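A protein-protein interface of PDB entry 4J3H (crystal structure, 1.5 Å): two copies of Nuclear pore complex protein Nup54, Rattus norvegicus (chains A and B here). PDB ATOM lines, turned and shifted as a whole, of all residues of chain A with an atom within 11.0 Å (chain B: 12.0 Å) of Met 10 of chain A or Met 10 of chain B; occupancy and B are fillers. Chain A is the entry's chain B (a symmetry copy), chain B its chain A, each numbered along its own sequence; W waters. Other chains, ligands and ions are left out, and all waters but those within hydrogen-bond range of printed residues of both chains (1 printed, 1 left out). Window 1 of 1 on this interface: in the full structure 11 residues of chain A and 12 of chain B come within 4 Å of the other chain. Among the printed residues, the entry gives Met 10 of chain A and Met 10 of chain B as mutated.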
ATOM      1  N   GLU A   5     -16.498 -23.177   2.406  1.00  0.00           N
ATOM      2  CA  GLU A   5     -16.181 -23.515   3.791  1.00  0.00           C
ATOM      3  C   GLU A   5     -14.834 -22.930   4.185  1.00  0.00           C
ATOM      4  O   GLU A   5     -13.789 -23.527   3.922  1.00  0.00           O
ATOM      5  N   GLU A   6     -14.862 -21.766   4.825  1.00  0.00           N
ATOM      6  CA  GLU A   6     -13.625 -21.055   5.184  1.00  0.00           C
ATOM      7  C   GLU A   6     -12.985 -21.649   6.424  1.00  0.00           C
ATOM      8  O   GLU A   6     -13.606 -21.718   7.483  1.00  0.00           O
ATOM      9  CB  GLU A   6     -13.919 -19.577   5.427  1.00  0.00           C
ATOM     10  CG  GLU A   6     -12.660 -18.752   5.520  1.00  0.00           C
ATOM     11  CD  GLU A   6     -12.940 -17.299   5.822  1.00  0.00           C
ATOM     12  OE1 GLU A   6     -13.817 -16.722   5.154  1.00  0.00           O
ATOM     13  OE2 GLU A   6     -12.288 -16.739   6.729  1.00  0.00           O
ATOM     14  N   LYS A   7     -11.745 -22.097   6.275  1.00  0.00           N
ATOM     15  CA  LYS A   7     -11.069 -22.803   7.355  1.00  0.00           C
ATOM     16  C   LYS A   7      -9.580 -22.547   7.269  1.00  0.00           C
ATOM     17  O   LYS A   7      -9.084 -22.064   6.244  1.00  0.00           O
ATOM     18  CB  LYS A   7     -11.364 -24.300   7.294  1.00  0.00           C
ATOM     19  CG  LYS A   7     -10.698 -24.969   6.120  1.00  0.00           C
ATOM     20  CD  LYS A   7     -11.318 -26.317   5.741  1.00  0.00           C
ATOM     21  CE  LYS A   7     -10.551 -26.886   4.558  1.00  0.00           C
ATOM     22  NZ  LYS A   7     -11.158 -28.091   3.933  1.00  0.00           N
ATOM     23  N   TYR A   8      -8.881 -22.879   8.340  1.00  0.00           N
ATOM     24  CA  TYR A   8      -7.491 -22.480   8.493  1.00  0.00           C
ATOM     25  C   TYR A   8      -6.633 -23.662   8.899  1.00  0.00           C
ATOM     26  O   TYR A   8      -6.862 -24.272   9.941  1.00  0.00           O
ATOM     27  CB  TYR A   8      -7.395 -21.351   9.540  1.00  0.00           C
ATOM     28  CG  TYR A   8      -8.009 -20.076   9.020  1.00  0.00           C
ATOM     29  CD1 TYR A   8      -9.381 -19.842   9.115  1.00  0.00           C
ATOM     30  CD2 TYR A   8      -7.229 -19.116   8.403  1.00  0.00           C
ATOM     31  CE1 TYR A   8      -9.953 -18.699   8.610  1.00  0.00           C
ATOM     32  CE2 TYR A   8      -7.800 -17.960   7.889  1.00  0.00           C
ATOM     33  CZ  TYR A   8      -9.157 -17.760   8.003  1.00  0.00           C
ATOM     34  OH  TYR A   8      -9.738 -16.625   7.496  1.00  0.00           O
ATOM     35  N   TYR A   9      -5.658 -23.984   8.051  1.00  0.00           N
ATOM     36  CA  TYR A   9      -4.644 -24.990   8.339  1.00  0.00           C
ATOM     37  C   TYR A   9      -3.798 -24.591   9.534  1.00  0.00           C
ATOM     38  O   TYR A   9      -3.376 -23.431   9.665  1.00  0.00           O
ATOM     39  CB  TYR A   9      -3.734 -25.094   7.110  1.00  0.00           C
ATOM     40  CG  TYR A   9      -2.616 -26.104   7.128  1.00  0.00           C
ATOM     41  CD1 TYR A   9      -2.871 -27.454   6.945  1.00  0.00           C
ATOM     42  CD2 TYR A   9      -1.289 -25.690   7.226  1.00  0.00           C
ATOM     43  CE1 TYR A   9      -1.832 -28.387   6.898  1.00  0.00           C
ATOM     44  CE2 TYR A   9      -0.252 -26.620   7.175  1.00  0.00           C
ATOM     45  CZ  TYR A   9      -0.543 -27.954   7.012  1.00  0.00           C
ATOM     46  OH  TYR A   9       0.469 -28.885   6.960  1.00  0.00           O
ATOM     47  N   MET A  10      -3.541 -25.552  10.422  1.00  0.00           N
ATOM     48  CA  MET A  10      -2.527 -25.312  11.446  1.00  0.00           C
ATOM     49  C   MET A  10      -1.931 -26.617  11.909  1.00  0.00           C
ATOM     50  O   MET A  10      -2.556 -27.683  11.794  1.00  0.00           O
ATOM     51  CB  MET A  10      -3.098 -24.541  12.618  1.00  0.00           C
ATOM     52  CG  MET A  10      -4.186 -25.298  13.299  1.00  0.00           C
ATOM     53  SD  MET A  10      -5.017 -24.277  14.755  1.00  0.00           S
ATOM     54  CE  MET A  10      -5.579 -22.773  13.684  1.00  0.00           C
ATOM     55  N   ASP A  11      -0.718 -26.547  12.424  1.00  0.00           N
ATOM     56  CA  ASP A  11      -0.118 -27.759  12.946  1.00  0.00           C
ATOM     57  C   ASP A  11      -0.553 -28.072  14.369  1.00  0.00           C
ATOM     58  O   ASP A  11      -1.161 -27.242  15.064  1.00  0.00           O
ATOM     59  CB  ASP A  11       1.414 -27.812  12.768  1.00  0.00           C
ATOM     60  CG  ASP A  11       2.148 -26.678  13.455  1.00  0.00           C
ATOM     61  OD1 ASP A  11       1.601 -26.027  14.370  1.00  0.00           O
ATOM     62  OD2 ASP A  11       3.325 -26.456  13.092  1.00  0.00           O
ATOM     63  N   ALA A  12      -0.295 -29.301  14.777  1.00  0.00           N
ATOM     64  CA  ALA A  12      -0.669 -29.751  16.106  1.00  0.00           C
ATOM     65  C   ALA A  12      -0.032 -28.862  17.160  1.00  0.00           C
ATOM     66  O   ALA A  12      -0.621 -28.645  18.208  1.00  0.00           O
ATOM     67  CB  ALA A  12      -0.253 -31.199  16.301  1.00  0.00           C
ATOM     68  N   ASP A  13       1.165 -28.358  16.888  1.00  0.00           N
ATOM     69  CA  ASP A  13       1.839 -27.520  17.887  1.00  0.00           C
ATOM     70  C   ASP A  13       1.042 -26.247  18.184  1.00  0.00           C
ATOM     71  O   ASP A  13       0.847 -25.855  19.347  1.00  0.00           O
ATOM     72  CB  ASP A  13       3.269 -27.169  17.433  1.00  0.00           C
ATOM     73  CG  ASP A  13       4.214 -28.372  17.438  1.00  0.00           C
ATOM     74  OD1 ASP A  13       4.048 -29.290  18.271  1.00  0.00           O
ATOM     75  OD2 ASP A  13       5.146 -28.384  16.605  1.00  0.00           O
ATOM     76  N   LEU A  14       0.552 -25.599  17.134  1.00  0.00           N
ATOM     77  CA  LEU A  14      -0.202 -24.376  17.332  1.00  0.00           C
ATOM     78  C   LEU A  14      -1.519 -24.684  18.040  1.00  0.00           C
ATOM     79  O   LEU A  14      -1.902 -23.981  18.969  1.00  0.00           O
ATOM     80  CB  LEU A  14      -0.419 -23.637  16.004  1.00  0.00           C
ATOM     81  CG  LEU A  14      -1.180 -22.320  16.171  1.00  0.00           C
ATOM     82  CD1 LEU A  14      -0.392 -21.368  17.042  1.00  0.00           C
ATOM     83  CD2 LEU A  14      -1.490 -21.692  14.807  1.00  0.00           C
ATOM     84  N   LEU A  15      -2.236 -25.716  17.619  1.00  0.00           N
ATOM     85  CA  LEU A  15      -3.497 -26.051  18.267  1.00  0.00           C
ATOM     86  C   LEU A  15      -3.259 -26.410  19.738  1.00  0.00           C
ATOM     87  O   LEU A  15      -4.038 -26.007  20.609  1.00  0.00           O
ATOM     88  CB  LEU A  15      -4.159 -27.205  17.532  1.00  0.00           C
ATOM     89  CG  LEU A  15      -5.473 -27.696  18.133  1.00  0.00           C
ATOM     90  CD1 LEU A  15      -6.451 -26.529  18.193  1.00  0.00           C
ATOM     91  CD2 LEU A  15      -6.002 -28.832  17.282  1.00  0.00           C
ATOM     92  N   ARG A  16      -2.162 -27.105  20.030  1.00  0.00           N
ATOM     93  CA  ARG A  16      -1.867 -27.455  21.419  1.00  0.00           C
ATOM     94  C   ARG A  16      -1.636 -26.194  22.259  1.00  0.00           C
ATOM     95  O   ARG A  16      -2.082 -26.103  23.408  1.00  0.00           O
ATOM     96  CB  ARG A  16      -0.645 -28.345  21.470  1.00  0.00           C
ATOM     97  CG  ARG A  16      -0.248 -28.720  22.894  1.00  0.00           C
ATOM     98  CD  ARG A  16       1.041 -29.523  22.933  1.00  0.00           C
ATOM     99  NE  ARG A  16       2.157 -28.788  22.344  1.00  0.00           N
ATOM    100  CZ  ARG A  16       2.745 -29.110  21.198  1.00  0.00           C
ATOM    101  NH1 ARG A  16       2.333 -30.168  20.508  1.00  0.00           N
ATOM    102  NH2 ARG A  16       3.754 -28.376  20.747  1.00  0.00           N
ATOM    103  N   GLU A  17      -0.922 -25.230  21.692  1.00  0.00           N
ATOM    104  CA  GLU A  17      -0.667 -23.993  22.434  1.00  0.00           C
ATOM    105  C   GLU A  17      -1.950 -23.211  22.692  1.00  0.00           C
ATOM    106  O   GLU A  17      -2.084 -22.602  23.758  1.00  0.00           O
ATOM    107  CB  GLU A  17       0.348 -23.101  21.716  1.00  0.00           C
ATOM    108  CG  GLU A  17       1.708 -23.729  21.556  1.00  0.00           C
ATOM    109  CD  GLU A  17       2.510 -23.759  22.853  1.00  0.00           C
ATOM    110  OE1 GLU A  17       2.120 -23.069  23.817  1.00  0.00           O
ATOM    111  OE2 GLU A  17       3.532 -24.477  22.918  1.00  0.00           O
ATOM    112  N   ILE A  18      -2.857 -23.188  21.714  1.00  0.00           N
ATOM    113  CA  ILE A  18      -4.145 -22.529  21.921  1.00  0.00           C
ATOM    114  C   ILE A  18      -4.904 -23.226  23.043  1.00  0.00           C
ATOM    115  O   ILE A  18      -5.384 -22.583  23.988  1.00  0.00           O
ATOM    116  CB  ILE A  18      -4.972 -22.563  20.642  1.00  0.00           C
ATOM    117  CG1 ILE A  18      -4.332 -21.640  19.605  1.00  0.00           C
ATOM    118  CG2 ILE A  18      -6.422 -22.180  20.957  1.00  0.00           C
ATOM    119  CD1 ILE A  18      -4.976 -21.714  18.190  1.00  0.00           C
ATOM    120  N   LYS A  19      -5.006 -24.548  22.957  1.00  0.00           N
ATOM    121  CA  LYS A  19      -5.712 -25.310  23.964  1.00  0.00           C
ATOM    122  C   LYS A  19      -5.113 -25.101  25.354  1.00  0.00           C
ATOM    123  O   LYS A  19      -5.848 -24.923  26.353  1.00  0.00           O
ATOM    124  CB  LYS A  19      -5.713 -26.788  23.591  1.00  0.00           C
ATOM    125  CG  LYS A  19      -6.671 -27.078  22.456  1.00  0.00           C
ATOM    126  CD  LYS A  19      -6.402 -28.441  21.850  1.00  0.00           C
ATOM    127  CE  LYS A  19      -6.517 -29.551  22.871  1.00  0.00           C
ATOM    128  NZ  LYS A  19      -6.128 -30.866  22.273  1.00  0.00           N
ATOM    129  N   GLN A  20      -3.784 -25.123  25.443  1.00  0.00           N
ATOM    130  CA  GLN A  20      -3.104 -24.979  26.726  1.00  0.00           C
ATOM    131  C   GLN A  20      -3.394 -23.610  27.333  1.00  0.00           C
ATOM    132  O   GLN A  20      -3.575 -23.497  28.553  1.00  0.00           O
ATOM    133  CB  GLN A  20      -1.605 -25.173  26.538  1.00  0.00           C
ATOM    134  CG  GLN A  20      -0.807 -25.259  27.799  1.00  0.00           C
ATOM    135  CD  GLN A  20       0.598 -25.710  27.493  1.00  0.00           C
ATOM    136  OE1 GLN A  20       0.873 -26.155  26.372  1.00  0.00           O
ATOM    137  NE2 GLN A  20       1.497 -25.598  28.469  1.00  0.00           N
ATOM    138  N   LEU A  22      -6.063 -21.684  26.913  1.00  0.00           N
ATOM    139  CA  LEU A  22      -7.423 -21.613  27.439  1.00  0.00           C
ATOM    140  C   LEU A  22      -7.543 -22.414  28.731  1.00  0.00           C
ATOM    141  O   LEU A  22      -8.178 -21.962  29.708  1.00  0.00           O
ATOM    142  CB  LEU A  22      -8.437 -22.095  26.394  1.00  0.00           C
ATOM    143  CG  LEU A  22      -8.359 -21.304  25.088  1.00  0.00           C
ATOM    144  CD1 LEU A  22      -9.414 -21.821  24.120  1.00  0.00           C
ATOM    145  CD2 LEU A  22      -8.534 -19.811  25.340  1.00  0.00           C
ATOM    146  N   GLU B   5      -2.922 -37.029  11.405  1.00  0.00           N
ATOM    147  CA  GLU B   5      -2.558 -37.241  12.802  1.00  0.00           C
ATOM    148  C   GLU B   5      -1.660 -36.120  13.313  1.00  0.00           C
ATOM    149  O   GLU B   5      -1.174 -36.168  14.447  1.00  0.00           O
ATOM    150  N   GLU B   6      -1.441 -35.108  12.478  1.00  0.00           N
ATOM    151  CA  GLU B   6      -0.488 -34.059  12.812  1.00  0.00           C
ATOM    152  C   GLU B   6      -0.937 -32.658  12.409  1.00  0.00           C
ATOM    153  O   GLU B   6      -0.406 -31.685  12.936  1.00  0.00           O
ATOM    154  CB  GLU B   6       0.909 -34.361  12.219  1.00  0.00           C
ATOM    155  CG  GLU B   6       1.928 -33.225  12.427  1.00  0.00           C
ATOM    156  N   LYS B   7      -1.881 -32.545  11.467  1.00  0.00           N
ATOM    157  CA  LYS B   7      -2.350 -31.226  11.005  1.00  0.00           C
ATOM    158  C   LYS B   7      -3.858 -31.113  11.125  1.00  0.00           C
ATOM    159  O   LYS B   7      -4.568 -32.121  11.016  1.00  0.00           O
ATOM    160  CB  LYS B   7      -1.954 -30.987   9.535  1.00  0.00           C
ATOM    161  CG  LYS B   7      -0.516 -31.319   9.210  1.00  0.00           C
ATOM    162  CD  LYS B   7       0.434 -30.311   9.784  1.00  0.00           C
ATOM    163  CE  LYS B   7       1.841 -30.781   9.462  1.00  0.00           C
ATOM    164  NZ  LYS B   7       2.852 -29.954  10.144  1.00  0.00           N
ATOM    165  N   TYR B   8      -4.345 -29.883  11.303  1.00  0.00           N
ATOM    166  CA  TYR B   8      -5.781 -29.652  11.518  1.00  0.00           C
ATOM    167  C   TYR B   8      -6.259 -28.503  10.676  1.00  0.00           C
ATOM    168  O   TYR B   8      -5.457 -27.648  10.286  1.00  0.00           O
ATOM    169  CB  TYR B   8      -6.027 -29.311  12.990  1.00  0.00           C
ATOM    170  CG  TYR B   8      -5.625 -30.442  13.881  1.00  0.00           C
ATOM    171  CD1 TYR B   8      -4.320 -30.563  14.337  1.00  0.00           C
ATOM    172  CD2 TYR B   8      -6.548 -31.409  14.233  1.00  0.00           C
ATOM    173  CE1 TYR B   8      -3.941 -31.641  15.140  1.00  0.00           C
ATOM    174  CE2 TYR B   8      -6.185 -32.485  15.024  1.00  0.00           C
ATOM    175  CZ  TYR B   8      -4.890 -32.588  15.477  1.00  0.00           C
ATOM    176  OH  TYR B   8      -4.536 -33.660  16.262  1.00  0.00           O
ATOM    177  N   TYR B   9      -7.567 -28.457  10.442  1.00  0.00           N
ATOM    178  CA  TYR B   9      -8.215 -27.266   9.916  1.00  0.00           C
ATOM    179  C   TYR B   9      -9.084 -26.711  11.018  1.00  0.00           C
ATOM    180  O   TYR B   9      -9.840 -27.469  11.629  1.00  0.00           O
ATOM    181  CB  TYR B   9      -9.148 -27.602   8.762  1.00  0.00           C
ATOM    182  CG  TYR B   9      -8.499 -28.158   7.527  1.00  0.00           C
ATOM    183  CD1 TYR B   9      -7.489 -27.461   6.863  1.00  0.00           C
ATOM    184  CD2 TYR B   9      -8.896 -29.376   7.008  1.00  0.00           C
ATOM    185  CE1 TYR B   9      -6.900 -27.987   5.704  1.00  0.00           C
ATOM    186  CE2 TYR B   9      -8.325 -29.898   5.861  1.00  0.00           C
ATOM    187  CZ  TYR B   9      -7.325 -29.205   5.213  1.00  0.00           C
ATOM    188  OH  TYR B   9      -6.766 -29.748   4.081  1.00  0.00           O
ATOM    189  N   MET B  10      -9.010 -25.410  11.266  1.00  0.00           N
ATOM    190  CA  MET B  10      -9.921 -24.748  12.202  1.00  0.00           C
ATOM    191  C   MET B  10     -10.916 -23.887  11.448  1.00  0.00           C
ATOM    192  O   MET B  10     -10.525 -23.119  10.568  1.00  0.00           O
ATOM    193  CB  MET B  10      -9.127 -23.843  13.152  1.00  0.00           C
ATOM    194  CG  MET B  10     -10.012 -23.202  14.223  1.00  0.00           C
ATOM    195  SD  MET B  10      -9.003 -22.167  15.511  1.00  0.00           S
ATOM    196  CE  MET B  10      -8.452 -23.639  16.641  1.00  0.00           C
ATOM    197  N   ASP B  11     -12.193 -23.996  11.803  1.00  0.00           N
ATOM    198  CA  ASP B  11     -13.212 -23.179  11.140  1.00  0.00           C
ATOM    199  C   ASP B  11     -12.984 -21.698  11.392  1.00  0.00           C
ATOM    200  O   ASP B  11     -12.519 -21.272  12.479  1.00  0.00           O
ATOM    201  CB  ASP B  11     -14.642 -23.533  11.608  1.00  0.00           C
ATOM    202  CG  ASP B  11     -15.228 -24.739  10.930  1.00  0.00           C
ATOM    203  OD1 ASP B  11     -14.517 -25.654  10.531  1.00  0.00           O
ATOM    204  OD2 ASP B  11     -16.467 -24.778  10.845  1.00  0.00           O
ATOM    205  N   ALA B  12     -13.382 -20.885  10.418  1.00  0.00           N
ATOM    206  CA  ALA B  12     -13.194 -19.445  10.480  1.00  0.00           C
ATOM    207  C   ALA B  12     -13.830 -18.802  11.708  1.00  0.00           C
ATOM    208  O   ALA B  12     -13.209 -17.923  12.332  1.00  0.00           O
ATOM    209  CB  ALA B  12     -13.746 -18.804   9.207  1.00  0.00           C
ATOM    210  N   ASP B  13     -15.034 -19.219  12.067  1.00  0.00           N
ATOM    211  CA  ASP B  13     -15.710 -18.590  13.199  1.00  0.00           C
ATOM    212  C   ASP B  13     -14.964 -18.827  14.509  1.00  0.00           C
ATOM    213  O   ASP B  13     -14.760 -17.892  15.298  1.00  0.00           O
ATOM    214  CB  ASP B  13     -17.223 -18.905  13.273  1.00  0.00           C
ATOM    215  CG  ASP B  13     -17.571 -20.377  13.223  1.00  0.00           C
ATOM    216  OD1 ASP B  13     -16.711 -21.280  13.291  1.00  0.00           O
ATOM    217  OD2 ASP B  13     -18.808 -20.640  13.147  1.00  0.00           O
ATOM    218  N   LEU B  14     -14.537 -20.059  14.751  1.00  0.00           N
ATOM    219  CA  LEU B  14     -13.772 -20.346  15.959  1.00  0.00           C
ATOM    220  C   LEU B  14     -12.473 -19.554  15.974  1.00  0.00           C
ATOM    221  O   LEU B  14     -12.123 -18.963  17.012  1.00  0.00           O
ATOM    222  CB  LEU B  14     -13.500 -21.850  16.080  1.00  0.00           C
ATOM    223  CG  LEU B  14     -12.596 -22.240  17.266  1.00  0.00           C
ATOM    224  CD1 LEU B  14     -13.125 -21.705  18.571  1.00  0.00           C
ATOM    225  CD2 LEU B  14     -12.445 -23.759  17.363  1.00  0.00           C
ATOM    226  N   LEU B  15     -11.769 -19.473  14.843  1.00  0.00           N
ATOM    227  CA  LEU B  15     -10.526 -18.695  14.853  1.00  0.00           C
ATOM    228  C   LEU B  15     -10.798 -17.225  15.144  1.00  0.00           C
ATOM    229  O   LEU B  15     -10.079 -16.604  15.950  1.00  0.00           O
ATOM    230  CB  LEU B  15      -9.753 -18.901  13.541  1.00  0.00           C
ATOM    231  CG  LEU B  15      -8.452 -18.114  13.452  1.00  0.00           C
ATOM    232  CD1 LEU B  15      -7.449 -18.599  14.507  1.00  0.00           C
ATOM    233  CD2 LEU B  15      -7.886 -18.254  12.024  1.00  0.00           C
ATOM    234  N   ARG B  16     -11.819 -16.672  14.507  1.00  0.00           N
ATOM    235  CA  ARG B  16     -12.189 -15.276  14.727  1.00  0.00           C
ATOM    236  C   ARG B  16     -12.448 -15.030  16.209  1.00  0.00           C
ATOM    237  O   ARG B  16     -11.975 -14.034  16.783  1.00  0.00           O
ATOM    238  CB  ARG B  16     -13.424 -14.942  13.897  1.00  0.00           C
ATOM    239  CG  ARG B  16     -13.990 -13.552  14.062  1.00  0.00           C
ATOM    240  CD  ARG B  16     -15.358 -13.492  13.406  1.00  0.00           C
ATOM    241  NE  ARG B  16     -16.367 -14.193  14.204  1.00  0.00           N
ATOM    242  CZ  ARG B  16     -17.307 -15.001  13.722  1.00  0.00           C
ATOM    243  NH1 ARG B  16     -17.383 -15.251  12.418  1.00  0.00           N
ATOM    244  NH2 ARG B  16     -18.182 -15.563  14.545  1.00  0.00           N
ATOM    245  N   GLU B  17     -13.196 -15.915  16.849  1.00  0.00           N
ATOM    246  CA  GLU B  17     -13.576 -15.672  18.242  1.00  0.00           C
ATOM    247  C   GLU B  17     -12.378 -15.837  19.149  1.00  0.00           C
ATOM    248  O   GLU B  17     -12.253 -15.099  20.128  1.00  0.00           O
ATOM    249  CB  GLU B  17     -14.734 -16.585  18.649  1.00  0.00           C
ATOM    250  CG  GLU B  17     -16.023 -16.287  17.863  1.00  0.00           C
ATOM    251  CD  GLU B  17     -16.490 -14.852  18.010  1.00  0.00           C
ATOM    252  OE1 GLU B  17     -16.724 -14.439  19.162  1.00  0.00           O
ATOM    253  OE2 GLU B  17     -16.646 -14.127  16.987  1.00  0.00           O
ATOM    254  N   ILE B  18     -11.484 -16.780  18.862  1.00  0.00           N
ATOM    255  CA  ILE B  18     -10.258 -16.905  19.641  1.00  0.00           C
ATOM    256  C   ILE B  18      -9.417 -15.639  19.537  1.00  0.00           C
ATOM    257  O   ILE B  18      -8.986 -15.099  20.556  1.00  0.00           O
ATOM    258  CB  ILE B  18      -9.451 -18.151  19.209  1.00  0.00           C
ATOM    259  CG1 ILE B  18     -10.169 -19.418  19.650  1.00  0.00           C
ATOM    260  CG2 ILE B  18      -8.048 -18.089  19.810  1.00  0.00           C
ATOM    261  CD1 ILE B  18      -9.555 -20.713  19.111  1.00  0.00           C
ATOM    262  N   LYS B  19      -9.187 -15.166  18.316  1.00  0.00           N
ATOM    263  CA  LYS B  19      -8.374 -13.952  18.150  1.00  0.00           C
ATOM    264  C   LYS B  19      -9.013 -12.789  18.892  1.00  0.00           C
ATOM    265  O   LYS B  19      -8.290 -12.014  19.537  1.00  0.00           O
ATOM    266  CB  LYS B  19      -8.254 -13.579  16.693  1.00  0.00           C
ATOM    267  CG  LYS B  19      -7.425 -14.544  15.872  1.00  0.00           C
ATOM    268  CD  LYS B  19      -7.273 -14.054  14.450  1.00  0.00           C
ATOM    269  CE  LYS B  19      -6.255 -14.868  13.716  1.00  0.00           C
ATOM    270  NZ  LYS B  19      -6.197 -14.456  12.290  1.00  0.00           N
ATOM    271  N   GLN B  20     -10.341 -12.657  18.823  1.00  0.00           N
ATOM    272  CA  GLN B  20     -11.015 -11.546  19.511  1.00  0.00           C
ATOM    273  C   GLN B  20     -10.805 -11.645  21.016  1.00  0.00           C
ATOM    274  O   GLN B  20     -10.556 -10.621  21.676  1.00  0.00           O
ATOM    275  CB  GLN B  20     -12.513 -11.512  19.165  1.00  0.00           C
ATOM    276  CG  GLN B  20     -13.281 -10.372  19.819  1.00  0.00           C
ATOM    277  CD  GLN B  20     -14.667 -10.204  19.220  1.00  0.00           C
ATOM    278  OE1 GLN B  20     -14.967 -10.764  18.161  1.00  0.00           O
ATOM    279  NE2 GLN B  20     -15.518  -9.442  19.893  1.00  0.00           N
ATOM    280  N   HIS B  21     -10.902 -12.853  21.566  1.00  0.00           N
ATOM    281  CA  HIS B  21     -10.705 -13.067  22.998  1.00  0.00           C
ATOM    282  C   HIS B  21      -9.297 -12.674  23.423  1.00  0.00           C
ATOM    283  O   HIS B  21      -9.106 -12.009  24.451  1.00  0.00           O
ATOM    284  CB  HIS B  21     -10.937 -14.551  23.348  1.00  0.00           C
ATOM    285  CG  HIS B  21     -10.689 -14.870  24.787  1.00  0.00           C
ATOM    286  ND1 HIS B  21     -11.611 -14.611  25.773  1.00  0.00           N
ATOM    287  CD2 HIS B  21      -9.595 -15.370  25.417  1.00  0.00           C
ATOM    288  CE1 HIS B  21     -11.108 -14.953  26.948  1.00  0.00           C
ATOM    289  NE2 HIS B  21      -9.891 -15.425  26.755  1.00  0.00           N
ATOM    290  N   LEU B  22      -8.304 -13.090  22.646  1.00  0.00           N
ATOM    291  CA  LEU B  22      -6.913 -12.814  23.001  1.00  0.00           C
ATOM    292  C   LEU B  22      -6.641 -11.318  22.949  1.00  0.00           C
ATOM    293  O   LEU B  22      -5.993 -10.763  23.850  1.00  0.00           O
ATOM    294  CB  LEU B  22      -5.947 -13.554  22.071  1.00  0.00           C
ATOM    295  CG  LEU B  22      -6.119 -15.067  22.071  1.00  0.00           C
ATOM    296  CD1 LEU B  22      -5.165 -15.642  21.064  1.00  0.00           C
ATOM    297  CD2 LEU B  22      -5.827 -15.639  23.448  1.00  0.00           C
HETATM  298  O   HOH W   1      -9.233 -28.986   2.445  1.00  0.00           O
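The backbone carbonyl oxygen (O) of Glu 6 of chain B lies within hydrogen-bond range of the backbone NH (N) of Ala 12 of chain A.
The backbone carbonyl oxygen (O) of Glu 6 of chain A is in hydrogen-bond range of the backbone NH (N) of Ala 12 of chain B, at 3.1 Å.
O of Tyr 8 of chain B lies within hydrogen-bond range of N of Met 10 of chain A (2.8 Å).
O of Tyr 8 of chain A sits at hydrogen-bond distance from N of Met 10 of chain B, at 2.8 Å.
N of Leu 14 of chain A is in hydrogen-bond range of OD1 of Asp 11 of chain A (3.0 Å).
The side-chain carboxylate (OE2) of Glu 6 of chain A is in hydrogen-bond range of the side-chain hydroxyl (OH) of Tyr 8 of chain A (2.7 Å).
N of Asp 13 of chain A lies close to OD1 of Asp 11 of chain A (3.5 Å).
Among the printed residues, merely in contact across the chains: Tyr 9 of chain A with Lys 7 of chain B, Lys 7 of chain A with Met 10 of chain B, Tyr 8 of chain A with Tyr 9 of chain B, Tyr 9 of chain A with Tyr 8 of chain B, Tyr 8 of chain A with Leu 15 of chain B, Met 10 of chain A with Lys 7 of chain B, Tyr 8 of chain A with Tyr 8 of chain B, Asp 11 of chain A with Lys 7 of chain B, Met 10 of chain A with Met 10 of chain B, Leu 15 of chain A with Tyr 8 of chain B, Lys 7 of chain A with Tyr 9 of chain B, Tyr 8 of chain A with Ala 12 of chain B, Leu 15 of chain A with Met 10 of chain B, Asp 11 of chain A with Glu 6 of chain B, Ala 12 of chain A with Tyr 8 of chain B, Ile 18 of chain A with Ile 18 of chain B and Glu 6 of chain A with Asp 11 of chain B.
Of the printed residues of chain B, Glu 6 of chain A touches Asp 11 and Ala 12.
Printed residues of chain B within 4 Å of Lys 7 of chain A: Tyr 9 (3.8 Å) and Met 10 (3.3 Å).
Printed residues of chain B within 4 Å of Tyr 8 of chain A: Tyr 8, Tyr 9, Met 10, Ala 12 and Leu 15.
Of chain B, only Lys 7 (3.2 Å) and Tyr 8 (3.4 Å) come within 4 Å of Tyr 9 of chain A.
Asp 11 of chain A touches just these residues of chain B: Glu 6 (3.9 Å) and Lys 7 (3.7 Å).
No residue of chain B comes within 4 Å of Leu 14 of chain A.
Leu 15 of chain A touches just these residues of chain B: Tyr 8 (3.8 Å) and Met 10 (3.8 Å).
Printed residues of chain B within 4 Å of Ile 18 of chain A: Ile 18.
Of the printed residues of chain A, Tyr 8 of chain B touches Tyr 8, Tyr 9, Met 10, Ala 12 and Leu 15.
Of the printed residues of chain A, Tyr 9 of chain B touches Lys 7 and Tyr 8.
Met 10 of chain B touches just these residues of chain A: Lys 7 (3.3 Å), Tyr 8 (2.8 Å), Met 10 (3.7 Å) and Leu 15 (3.8 Å).
Of chain A, only Glu 6 (3.96 Å) comes within 4 Å of Asp 11 of chain B.
Ala 12 of chain B touches just these residues of chain A: Glu 6 and Tyr 8.
No residue of chain A comes within 4 Å of Leu 14 of chain B.
His 21 of chain B touches none of the printed residues of chain A.
Of the 17 printed residues of chain A, 9 touch a printed residue of chain B.
Hydrophobic or aromatic side chains of chain B within 4 Å of the printed part of chain A: Tyr 8, Tyr 9, Met 10, Ala 12, Leu 15 and Ile 18.
Among the printed residues, 21 pairs touch across the chains.
Among the printed residues, no Asp or Glu carboxylate lies within 4 Å of a Lys or Arg side-chain nitrogen of the other chain.
Tyr 8 of chain A touches Leu 15 of chain B, and with the chains exchanged Leu 15 of chain A touches Tyr 8 of chain B.
Met 10 of chain A touches its own counterpart, Met 10 of chain B.
Leu 15 of chain A touches Met 10 of chain B, but with the chains exchanged Met 10 of chain A does not touch Leu 15 of chain B (4.6 Å).
Positions printed for both chains: 5, 6, 7, 8, 9, 10, 11, 12, 13, 14, 15, 16, 17, 18, 19, 20 and 22.
Of the 21 pairs that touch across the chains among the printed residues, 19 have their exchanged pair printed and touching as well.
Water W1 bridges NZ of Lys 7 of chain A (2.6 Å) and OH of Tyr 9 of chain B (3.1 Å).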
